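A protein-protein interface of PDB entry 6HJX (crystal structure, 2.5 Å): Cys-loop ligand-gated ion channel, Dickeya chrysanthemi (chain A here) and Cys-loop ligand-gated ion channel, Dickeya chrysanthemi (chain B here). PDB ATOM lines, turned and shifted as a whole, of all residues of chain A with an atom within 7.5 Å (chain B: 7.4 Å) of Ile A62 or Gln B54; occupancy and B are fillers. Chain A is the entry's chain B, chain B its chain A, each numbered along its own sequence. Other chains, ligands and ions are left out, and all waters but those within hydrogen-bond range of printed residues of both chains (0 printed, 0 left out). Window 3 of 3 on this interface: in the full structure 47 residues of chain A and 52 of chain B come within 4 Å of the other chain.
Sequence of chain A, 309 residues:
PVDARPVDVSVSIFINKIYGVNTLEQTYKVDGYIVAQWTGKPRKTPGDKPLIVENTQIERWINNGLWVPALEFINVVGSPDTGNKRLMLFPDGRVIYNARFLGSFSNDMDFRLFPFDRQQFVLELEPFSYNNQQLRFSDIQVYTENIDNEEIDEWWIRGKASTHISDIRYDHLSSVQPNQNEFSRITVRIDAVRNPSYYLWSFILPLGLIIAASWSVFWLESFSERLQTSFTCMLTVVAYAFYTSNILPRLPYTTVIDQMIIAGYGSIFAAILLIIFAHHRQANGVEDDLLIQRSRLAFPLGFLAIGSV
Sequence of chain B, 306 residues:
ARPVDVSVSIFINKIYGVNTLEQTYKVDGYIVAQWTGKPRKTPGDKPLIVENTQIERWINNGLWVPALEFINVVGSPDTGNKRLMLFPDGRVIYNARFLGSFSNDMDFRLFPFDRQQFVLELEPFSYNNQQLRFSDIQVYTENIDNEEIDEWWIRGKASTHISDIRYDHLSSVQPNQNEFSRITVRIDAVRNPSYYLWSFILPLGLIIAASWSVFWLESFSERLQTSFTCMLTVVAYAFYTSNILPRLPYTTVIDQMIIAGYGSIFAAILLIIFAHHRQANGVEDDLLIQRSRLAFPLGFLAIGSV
Glu A59 touches Thr B53.
Gln B54 touches Ile A62 (NE2 to CG2, 3.4 Å).
Glu B51 touches Pro A69 (OE1 to CA, 3.97 Å).
The side-chain amide oxygen (OE1) of Gln B54 lies within hydrogen-bond range of the guanidinium group (NH1) of Arg B57, at 3.0 Å.
ND2 of Asn A63 lies within hydrogen-bond range of O of Glu A59 (3.2 Å).
Printed residues of chain A that touch a printed residue of chain B: Glu A59, Ile A62, Asn A63 and Pro A69.
Hydrophobic or aromatic side chains of chain A within 4 Å of the printed part of chain B: Ile A62.
Of the 13 printed residues of chain B, 4 touch a printed residue of chain A.
Printed residues of chain B that touch a printed residue of chain A: Glu B51, Thr B53, Gln B54 and Arg B57.
Among the printed residues, 6 pairs touch across the chains.
Among the printed residues, no Asp or Glu carboxylate lies within 4 Å of a Lys or Arg side-chain nitrogen of the other chain.
The side-chain carboxylate of Glu A59 sits at hydrogen-bond distance from the side-chain amide nitrogen of Gln B54, at 3.0 Å.
OD1 of Asn A63 lies within hydrogen-bond range of NE2 of Gln B54 (2.7 Å).
The guanidinium group of Arg B57 sits at hydrogen-bond distance from the backbone carbonyl oxygen of Asn A63 (2.7 Å).
Ile A62 touches one residue of chain B.
Trp A67 touches none of the printed residues of chain B.
Printed residues of chain B within 4 Å of Pro A69: Glu B51 (3.97 Å).
Printed residues of chain A within 4 Å of Glu B51: Pro A69.
Of the printed residues of chain A, Thr B53 touches Glu A59.
Gln B54 touches just these residues of chain A: Glu A59, Ile A62 and Asn A63.
Ile B59 touches none of the printed residues of chain A.
The nearest residue of chain B that does not touch Ile A62 is Arg B57 (4.6 Å).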
ATOM      1  N   GLN A  57      -9.567 -29.115 -25.605  1.00  0.00           N
ATOM      2  CA  GLN A  57     -10.834 -29.822 -25.462  1.00  0.00           C
ATOM      3  C   GLN A  57     -11.686 -29.235 -24.348  1.00  0.00           C
ATOM      4  O   GLN A  57     -12.901 -29.457 -24.327  1.00  0.00           O
ATOM      5  CB  GLN A  57     -10.589 -31.308 -25.197  1.00  0.00           C
ATOM      6  CG  GLN A  57      -9.973 -32.047 -26.364  1.00  0.00           C
ATOM      7  CD  GLN A  57     -10.807 -31.931 -27.618  1.00  0.00           C
ATOM      8  OE1 GLN A  57     -11.896 -32.496 -27.710  1.00  0.00           O
ATOM      9  NE2 GLN A  57     -10.307 -31.180 -28.591  1.00  0.00           N
ATOM     10  N   ILE A  58     -11.074 -28.494 -23.422  1.00  0.00           N
ATOM     11  CA  ILE A  58     -11.833 -27.871 -22.345  1.00  0.00           C
ATOM     12  C   ILE A  58     -12.826 -26.862 -22.911  1.00  0.00           C
ATOM     13  O   ILE A  58     -13.975 -26.781 -22.461  1.00  0.00           O
ATOM     14  CB  ILE A  58     -10.868 -27.231 -21.327  1.00  0.00           C
ATOM     15  CG1 ILE A  58     -10.027 -28.327 -20.657  1.00  0.00           C
ATOM     16  CG2 ILE A  58     -11.630 -26.429 -20.278  1.00  0.00           C
ATOM     17  CD1 ILE A  58      -8.902 -27.810 -19.776  1.00  0.00           C
ATOM     18  N   GLU A  59     -12.409 -26.090 -23.920  1.00  0.00           N
ATOM     19  CA  GLU A  59     -13.290 -25.068 -24.474  1.00  0.00           C
ATOM     20  C   GLU A  59     -14.497 -25.685 -25.169  1.00  0.00           C
ATOM     21  O   GLU A  59     -15.564 -25.062 -25.224  1.00  0.00           O
ATOM     22  CB  GLU A  59     -12.519 -24.175 -25.447  1.00  0.00           C
ATOM     23  CG  GLU A  59     -13.264 -22.911 -25.847  1.00  0.00           C
ATOM     24  CD  GLU A  59     -13.494 -21.977 -24.675  1.00  0.00           C
ATOM     25  OE1 GLU A  59     -12.665 -21.981 -23.742  1.00  0.00           O
ATOM     26  OE2 GLU A  59     -14.508 -21.245 -24.687  1.00  0.00           O
ATOM     27  N   ARG A  60     -14.351 -26.899 -25.706  1.00  0.00           N
ATOM     28  CA  ARG A  60     -15.501 -27.584 -26.290  1.00  0.00           C
ATOM     29  C   ARG A  60     -16.530 -27.932 -25.220  1.00  0.00           C
ATOM     30  O   ARG A  60     -17.739 -27.820 -25.452  1.00  0.00           O
ATOM     31  CB  ARG A  60     -15.041 -28.838 -27.037  1.00  0.00           C
ATOM     32  CG  ARG A  60     -14.125 -28.539 -28.222  1.00  0.00           C
ATOM     33  CD  ARG A  60     -13.623 -29.799 -28.925  1.00  0.00           C
ATOM     34  NE  ARG A  60     -14.644 -30.454 -29.744  1.00  0.00           N
ATOM     35  CZ  ARG A  60     -15.250 -31.602 -29.439  1.00  0.00           C
ATOM     36  NH1 ARG A  60     -14.956 -32.258 -28.324  1.00  0.00           N
ATOM     37  NH2 ARG A  60     -16.159 -32.100 -30.265  1.00  0.00           N
ATOM     38  N   TRP A  61     -16.069 -28.346 -24.035  1.00  0.00           N
ATOM     39  CA  TRP A  61     -16.987 -28.622 -22.937  1.00  0.00           C
ATOM     40  C   TRP A  61     -17.633 -27.347 -22.408  1.00  0.00           C
ATOM     41  O   TRP A  61     -18.780 -27.380 -21.949  1.00  0.00           O
ATOM     42  CB  TRP A  61     -16.254 -29.348 -21.809  1.00  0.00           C
ATOM     43  CG  TRP A  61     -16.067 -30.811 -22.071  1.00  0.00           C
ATOM     44  CD1 TRP A  61     -15.123 -31.388 -22.870  1.00  0.00           C
ATOM     45  CD2 TRP A  61     -16.845 -31.884 -21.530  1.00  0.00           C
ATOM     46  NE1 TRP A  61     -15.266 -32.754 -22.862  1.00  0.00           N
ATOM     47  CE2 TRP A  61     -16.317 -33.084 -22.046  1.00  0.00           C
ATOM     48  CE3 TRP A  61     -17.938 -31.948 -20.660  1.00  0.00           C
ATOM     49  CZ2 TRP A  61     -16.844 -34.332 -21.721  1.00  0.00           C
ATOM     50  CZ3 TRP A  61     -18.462 -33.190 -20.339  1.00  0.00           C
ATOM     51  CH2 TRP A  61     -17.915 -34.363 -20.868  1.00  0.00           C
ATOM     52  N   ILE A  62     -16.921 -26.221 -22.454  1.00  0.00           N
ATOM     53  CA  ILE A  62     -17.505 -24.961 -22.010  1.00  0.00           C
ATOM     54  C   ILE A  62     -18.624 -24.540 -22.954  1.00  0.00           C
ATOM     55  O   ILE A  62     -19.722 -24.175 -22.518  1.00  0.00           O
ATOM     56  CB  ILE A  62     -16.416 -23.879 -21.890  1.00  0.00           C
ATOM     57  CG1 ILE A  62     -15.464 -24.223 -20.738  1.00  0.00           C
ATOM     58  CG2 ILE A  62     -17.035 -22.498 -21.679  1.00  0.00           C
ATOM     59  CD1 ILE A  62     -14.258 -23.305 -20.624  1.00  0.00           C
ATOM     60  N   ASN A  63     -18.368 -24.600 -24.264  1.00  0.00           N
ATOM     61  CA  ASN A  63     -19.390 -24.214 -25.232  1.00  0.00           C
ATOM     62  C   ASN A  63     -20.676 -25.011 -25.046  1.00  0.00           C
ATOM     63  O   ASN A  63     -21.769 -24.489 -25.295  1.00  0.00           O
ATOM     64  CB  ASN A  63     -18.861 -24.393 -26.656  1.00  0.00           C
ATOM     65  CG  ASN A  63     -17.806 -23.368 -27.015  1.00  0.00           C
ATOM     66  OD1 ASN A  63     -17.854 -22.227 -26.560  1.00  0.00           O
ATOM     67  ND2 ASN A  63     -16.842 -23.772 -27.836  1.00  0.00           N
ATOM     68  N   ASN A  64     -20.576 -26.262 -24.602  1.00  0.00           N
ATOM     69  CA  ASN A  64     -21.744 -27.113 -24.427  1.00  0.00           C
ATOM     70  C   ASN A  64     -22.355 -27.009 -23.033  1.00  0.00           C
ATOM     71  O   ASN A  64     -23.264 -27.784 -22.714  1.00  0.00           O
ATOM     72  CB  ASN A  64     -21.387 -28.572 -24.731  1.00  0.00           C
ATOM     73  CG  ASN A  64     -21.331 -28.859 -26.223  1.00  0.00           C
ATOM     74  OD1 ASN A  64     -21.955 -28.163 -27.025  1.00  0.00           O
ATOM     75  ND2 ASN A  64     -20.584 -29.890 -26.599  1.00  0.00           N
ATOM     76  N   GLY A  65     -21.881 -26.088 -22.200  1.00  0.00           N
ATOM     77  CA  GLY A  65     -22.561 -25.750 -20.969  1.00  0.00           C
ATOM     78  C   GLY A  65     -21.845 -26.102 -19.682  1.00  0.00           C
ATOM     79  O   GLY A  65     -22.428 -25.919 -18.609  1.00  0.00           O
ATOM     80  N   LEU A  66     -20.610 -26.597 -19.740  1.00  0.00           N
ATOM     81  CA  LEU A  66     -19.875 -26.858 -18.507  1.00  0.00           C
ATOM     82  C   LEU A  66     -19.438 -25.542 -17.874  1.00  0.00           C
ATOM     83  O   LEU A  66     -18.954 -24.633 -18.556  1.00  0.00           O
ATOM     84  CB  LEU A  66     -18.657 -27.742 -18.771  1.00  0.00           C
ATOM     85  CG  LEU A  66     -17.838 -28.102 -17.525  1.00  0.00           C
ATOM     86  CD1 LEU A  66     -18.647 -28.975 -16.577  1.00  0.00           C
ATOM     87  CD2 LEU A  66     -16.534 -28.787 -17.902  1.00  0.00           C
ATOM     88  N   TRP A  67     -19.617 -25.442 -16.561  1.00  0.00           N
ATOM     89  CA  TRP A  67     -19.297 -24.226 -15.824  1.00  0.00           C
ATOM     90  C   TRP A  67     -17.862 -24.302 -15.316  1.00  0.00           C
ATOM     91  O   TRP A  67     -17.521 -25.196 -14.533  1.00  0.00           O
ATOM     92  CB  TRP A  67     -20.270 -24.031 -14.661  1.00  0.00           C
ATOM     93  CG  TRP A  67     -20.127 -22.713 -13.965  1.00  0.00           C
ATOM     94  CD1 TRP A  67     -20.406 -21.479 -14.480  1.00  0.00           C
ATOM     95  CD2 TRP A  67     -19.684 -22.495 -12.621  1.00  0.00           C
ATOM     96  NE1 TRP A  67     -20.157 -20.506 -13.542  1.00  0.00           N
ATOM     97  CE2 TRP A  67     -19.714 -21.104 -12.391  1.00  0.00           C
ATOM     98  CE3 TRP A  67     -19.262 -23.339 -11.589  1.00  0.00           C
ATOM     99  CZ2 TRP A  67     -19.341 -20.540 -11.175  1.00  0.00           C
ATOM    100  CZ3 TRP A  67     -18.889 -22.775 -10.380  1.00  0.00           C
ATOM    101  CH2 TRP A  67     -18.929 -21.389 -10.184  1.00  0.00           C
ATOM    102  N   VAL A  68     -17.032 -23.363 -15.761  1.00  0.00           N
ATOM    103  CA  VAL A  68     -15.640 -23.271 -15.322  1.00  0.00           C
ATOM    104  C   VAL A  68     -15.348 -21.809 -15.004  1.00  0.00           C
ATOM    105  O   VAL A  68     -15.021 -21.035 -15.916  1.00  0.00           O
ATOM    106  CB  VAL A  68     -14.670 -23.803 -16.389  1.00  0.00           C
ATOM    107  CG1 VAL A  68     -13.257 -23.905 -15.818  1.00  0.00           C
ATOM    108  CG2 VAL A  68     -15.131 -25.149 -16.917  1.00  0.00           C
ATOM    109  N   PRO A  69     -15.450 -21.384 -13.747  1.00  0.00           N
ATOM    110  CA  PRO A  69     -15.290 -19.958 -13.442  1.00  0.00           C
ATOM    111  C   PRO A  69     -13.845 -19.506 -13.581  1.00  0.00           C
ATOM    112  O   PRO A  69     -12.904 -20.249 -13.294  1.00  0.00           O
ATOM    113  CB  PRO A  69     -15.770 -19.852 -11.992  1.00  0.00           C
ATOM    114  CG  PRO A  69     -15.473 -21.190 -11.418  1.00  0.00           C
ATOM    115  CD  PRO A  69     -15.690 -22.180 -12.530  1.00  0.00           C
ATOM    116  N   LYS A  85      -3.208 -27.497 -19.303  1.00  0.00           N
ATOM    117  CA  LYS A  85      -4.319 -27.414 -18.363  1.00  0.00           C
ATOM    118  C   LYS A  85      -5.209 -28.636 -18.546  1.00  0.00           C
ATOM    119  O   LYS A  85      -5.235 -29.264 -19.608  1.00  0.00           O
ATOM    120  CB  LYS A  85      -5.118 -26.110 -18.518  1.00  0.00           C
ATOM    121  CG  LYS A  85      -5.447 -25.688 -19.937  1.00  0.00           C
ATOM    122  CD  LYS A  85      -5.744 -24.190 -19.975  1.00  0.00           C
ATOM    123  CE  LYS A  85      -6.139 -23.710 -21.364  1.00  0.00           C
ATOM    124  NZ  LYS A  85      -7.509 -24.149 -21.744  1.00  0.00           N
ATOM    125  N   LEU A  87      -8.985 -30.750 -17.010  1.00  0.00           N
ATOM    126  CA  LEU A  87     -10.183 -30.934 -16.206  1.00  0.00           C
ATOM    127  C   LEU A  87     -10.329 -32.422 -15.924  1.00  0.00           C
ATOM    128  O   LEU A  87     -10.199 -33.243 -16.840  1.00  0.00           O
ATOM    129  CB  LEU A  87     -11.439 -30.418 -16.915  1.00  0.00           C
ATOM    130  CG  LEU A  87     -11.630 -28.913 -17.082  1.00  0.00           C
ATOM    131  CD1 LEU A  87     -12.969 -28.653 -17.750  1.00  0.00           C
ATOM    132  CD2 LEU A  87     -11.548 -28.189 -15.748  1.00  0.00           C
ATOM    133  N   ILE B  49     -23.710 -13.706 -16.443  1.00  0.00           N
ATOM    134  CA  ILE B  49     -22.276 -13.477 -16.557  1.00  0.00           C
ATOM    135  C   ILE B  49     -21.754 -14.292 -17.729  1.00  0.00           C
ATOM    136  O   ILE B  49     -22.039 -15.491 -17.840  1.00  0.00           O
ATOM    137  CB  ILE B  49     -21.551 -13.843 -15.250  1.00  0.00           C
ATOM    138  CG1 ILE B  49     -21.764 -12.725 -14.222  1.00  0.00           C
ATOM    139  CG2 ILE B  49     -20.059 -14.099 -15.504  1.00  0.00           C
ATOM    140  CD1 ILE B  49     -21.210 -13.021 -12.849  1.00  0.00           C
ATOM    141  N   VAL B  50     -21.007 -13.640 -18.613  1.00  0.00           N
ATOM    142  CA  VAL B  50     -20.351 -14.293 -19.737  1.00  0.00           C
ATOM    143  C   VAL B  50     -18.883 -13.896 -19.697  1.00  0.00           C
ATOM    144  O   VAL B  50     -18.564 -12.707 -19.590  1.00  0.00           O
ATOM    145  CB  VAL B  50     -20.988 -13.900 -21.082  1.00  0.00           C
ATOM    146  CG1 VAL B  50     -20.405 -14.740 -22.204  1.00  0.00           C
ATOM    147  CG2 VAL B  50     -22.511 -14.047 -21.022  1.00  0.00           C
ATOM    148  N   GLU B  51     -17.995 -14.885 -19.773  1.00  0.00           N
ATOM    149  CA  GLU B  51     -16.569 -14.674 -19.560  1.00  0.00           C
ATOM    150  C   GLU B  51     -15.771 -15.064 -20.796  1.00  0.00           C
ATOM    151  O   GLU B  51     -15.967 -16.145 -21.357  1.00  0.00           O
ATOM    152  CB  GLU B  51     -16.076 -15.481 -18.357  1.00  0.00           C
ATOM    153  CG  GLU B  51     -16.490 -14.905 -17.024  1.00  0.00           C
ATOM    154  CD  GLU B  51     -15.965 -15.710 -15.858  1.00  0.00           C
ATOM    155  OE1 GLU B  51     -15.972 -16.956 -15.946  1.00  0.00           O
ATOM    156  OE2 GLU B  51     -15.534 -15.099 -14.859  1.00  0.00           O
ATOM    157  N   ASN B  52     -14.875 -14.168 -21.212  1.00  0.00           N
ATOM    158  CA  ASN B  52     -13.820 -14.479 -22.169  1.00  0.00           C
ATOM    159  C   ASN B  52     -14.342 -15.104 -23.458  1.00  0.00           C
ATOM    160  O   ASN B  52     -15.020 -14.434 -24.242  1.00  0.00           O
ATOM    161  CB  ASN B  52     -12.790 -15.393 -21.498  1.00  0.00           C
ATOM    162  CG  ASN B  52     -12.057 -14.705 -20.364  1.00  0.00           C
ATOM    163  OD1 ASN B  52     -11.640 -13.553 -20.492  1.00  0.00           O
ATOM    164  ND2 ASN B  52     -11.903 -15.402 -19.245  1.00  0.00           N
ATOM    165  N   THR B  53     -14.025 -16.381 -23.696  1.00  0.00           N
ATOM    166  CA  THR B  53     -14.298 -16.983 -24.999  1.00  0.00           C
ATOM    167  C   THR B  53     -15.790 -17.033 -25.305  1.00  0.00           C
ATOM    168  O   THR B  53     -16.180 -17.042 -26.479  1.00  0.00           O
ATOM    169  CB  THR B  53     -13.711 -18.394 -25.065  1.00  0.00           C
ATOM    170  OG1 THR B  53     -12.311 -18.351 -24.767  1.00  0.00           O
ATOM    171  CG2 THR B  53     -13.905 -18.991 -26.451  1.00  0.00           C
ATOM    172  N   GLN B  54     -16.636 -17.081 -24.276  1.00  0.00           N
ATOM    173  CA  GLN B  54     -18.074 -17.133 -24.501  1.00  0.00           C
ATOM    174  C   GLN B  54     -18.645 -15.787 -24.921  1.00  0.00           C
ATOM    175  O   GLN B  54     -19.743 -15.743 -25.484  1.00  0.00           O
ATOM    176  CB  GLN B  54     -18.786 -17.630 -23.242  1.00  0.00           C
ATOM    177  CG  GLN B  54     -18.374 -19.033 -22.834  1.00  0.00           C
ATOM    178  CD  GLN B  54     -18.569 -20.044 -23.948  1.00  0.00           C
ATOM    179  OE1 GLN B  54     -19.698 -20.361 -24.323  1.00  0.00           O
ATOM    180  NE2 GLN B  54     -17.465 -20.547 -24.491  1.00  0.00           N
ATOM    181  N   ILE B  55     -17.927 -14.692 -24.666  1.00  0.00           N
ATOM    182  CA  ILE B  55     -18.377 -13.385 -25.136  1.00  0.00           C
ATOM    183  C   ILE B  55     -18.545 -13.400 -26.651  1.00  0.00           C
ATOM    184  O   ILE B  55     -19.555 -12.932 -27.187  1.00  0.00           O
ATOM    185  CB  ILE B  55     -17.395 -12.287 -24.685  1.00  0.00           C
ATOM    186  CG1 ILE B  55     -17.433 -12.142 -23.162  1.00  0.00           C
ATOM    187  CG2 ILE B  55     -17.723 -10.958 -25.363  1.00  0.00           C
ATOM    188  CD1 ILE B  55     -16.378 -11.206 -22.605  1.00  0.00           C
ATOM    189  N   GLU B  56     -17.557 -13.949 -27.363  1.00  0.00           N
ATOM    190  CA  GLU B  56     -17.614 -13.954 -28.821  1.00  0.00           C
ATOM    191  C   GLU B  56     -18.863 -14.666 -29.322  1.00  0.00           C
ATOM    192  O   GLU B  56     -19.510 -14.205 -30.270  1.00  0.00           O
ATOM    193  CB  GLU B  56     -16.361 -14.614 -29.395  1.00  0.00           C
ATOM    194  CG  GLU B  56     -16.271 -14.533 -30.909  1.00  0.00           C
ATOM    195  CD  GLU B  56     -16.207 -13.102 -31.410  1.00  0.00           C
ATOM    196  OE1 GLU B  56     -15.864 -12.205 -30.610  1.00  0.00           O
ATOM    197  OE2 GLU B  56     -16.499 -12.871 -32.604  1.00  0.00           O
ATOM    198  N   ARG B  57     -19.216 -15.793 -28.702  1.00  0.00           N
ATOM    199  CA  ARG B  57     -20.411 -16.516 -29.120  1.00  0.00           C
ATOM    200  C   ARG B  57     -21.641 -15.619 -29.075  1.00  0.00           C
ATOM    201  O   ARG B  57     -22.522 -15.716 -29.937  1.00  0.00           O
ATOM    202  CB  ARG B  57     -20.617 -17.745 -28.234  1.00  0.00           C
ATOM    203  CG  ARG B  57     -19.587 -18.849 -28.440  1.00  0.00           C
ATOM    204  CD  ARG B  57     -19.961 -20.100 -27.655  1.00  0.00           C
ATOM    205  NE  ARG B  57     -21.299 -20.580 -27.994  1.00  0.00           N
ATOM    206  CZ  ARG B  57     -21.999 -21.444 -27.264  1.00  0.00           C
ATOM    207  NH1 ARG B  57     -21.499 -21.931 -26.138  1.00  0.00           N
ATOM    208  NH2 ARG B  57     -23.207 -21.816 -27.659  1.00  0.00           N
ATOM    209  N   TRP B  58     -21.717 -14.736 -28.076  1.00  0.00           N
ATOM    210  CA  TRP B  58     -22.881 -13.868 -27.940  1.00  0.00           C
ATOM    211  C   TRP B  58     -22.912 -12.805 -29.029  1.00  0.00           C
ATOM    212  O   TRP B  58     -23.987 -12.456 -29.532  1.00  0.00           O
ATOM    213  CB  TRP B  58     -22.892 -13.216 -26.558  1.00  0.00           C
ATOM    214  CG  TRP B  58     -23.456 -14.093 -25.490  1.00  0.00           C
ATOM    215  CD1 TRP B  58     -22.810 -15.091 -24.818  1.00  0.00           C
ATOM    216  CD2 TRP B  58     -24.786 -14.051 -24.966  1.00  0.00           C
ATOM    217  NE1 TRP B  58     -23.657 -15.672 -23.908  1.00  0.00           N
ATOM    218  CE2 TRP B  58     -24.876 -15.051 -23.979  1.00  0.00           C
ATOM    219  CE3 TRP B  58     -25.909 -13.264 -25.235  1.00  0.00           C
ATOM    220  CZ2 TRP B  58     -26.045 -15.286 -23.263  1.00  0.00           C
ATOM    221  CZ3 TRP B  58     -27.070 -13.498 -24.521  1.00  0.00           C
ATOM    222  CH2 TRP B  58     -27.128 -14.500 -23.546  1.00  0.00           C
ATOM    223  N   ILE B  59     -21.748 -12.269 -29.402  1.00  0.00           N
ATOM    224  CA  ILE B  59     -21.710 -11.260 -30.456  1.00  0.00           C
ATOM    225  C   ILE B  59     -22.248 -11.838 -31.759  1.00  0.00           C
ATOM    226  O   ILE B  59     -23.047 -11.199 -32.456  1.00  0.00           O
ATOM    227  CB  ILE B  59     -20.280 -10.708 -30.618  1.00  0.00           C
ATOM    228  CG1 ILE B  59     -19.826 -10.043 -29.314  1.00  0.00           C
ATOM    229  CG2 ILE B  59     -20.219  -9.710 -31.768  1.00  0.00           C
ATOM    230  CD1 ILE B  59     -18.375  -9.609 -29.298  1.00  0.00           C
ATOM    231  N   LEU B  63     -25.510  -9.736 -29.967  1.00  0.00           N
ATOM    232  CA  LEU B  63     -25.151  -8.809 -28.901  1.00  0.00           C
ATOM    233  C   LEU B  63     -24.183  -7.751 -29.418  1.00  0.00           C
ATOM    234  O   LEU B  63     -23.242  -8.052 -30.157  1.00  0.00           O
ATOM    235  CB  LEU B  63     -24.526  -9.561 -27.724  1.00  0.00           C
ATOM    236  CG  LEU B  63     -24.220  -8.719 -26.481  1.00  0.00           C
ATOM    237  CD1 LEU B  63     -25.505  -8.335 -25.759  1.00  0.00           C
ATOM    238  CD2 LEU B  63     -23.276  -9.457 -25.541  1.00  0.00           C
ATOM    239  N   LEU B  84     -18.801 -10.000 -19.378  1.00  0.00           N
ATOM    240  CA  LEU B  84     -20.041  -9.280 -19.615  1.00  0.00           C
ATOM    241  C   LEU B  84     -21.039  -9.682 -18.543  1.00  0.00           C
ATOM    242  O   LEU B  84     -21.167 -10.870 -18.227  1.00  0.00           O
ATOM    243  CB  LEU B  84     -20.619  -9.584 -20.999  1.00  0.00           C
ATOM    244  CG  LEU B  84     -19.812  -9.126 -22.212  1.00  0.00           C
ATOM    245  CD1 LEU B  84     -20.521  -9.551 -23.478  1.00  0.00           C
ATOM    246  CD2 LEU B  84     -19.604  -7.621 -22.201  1.00  0.00           C
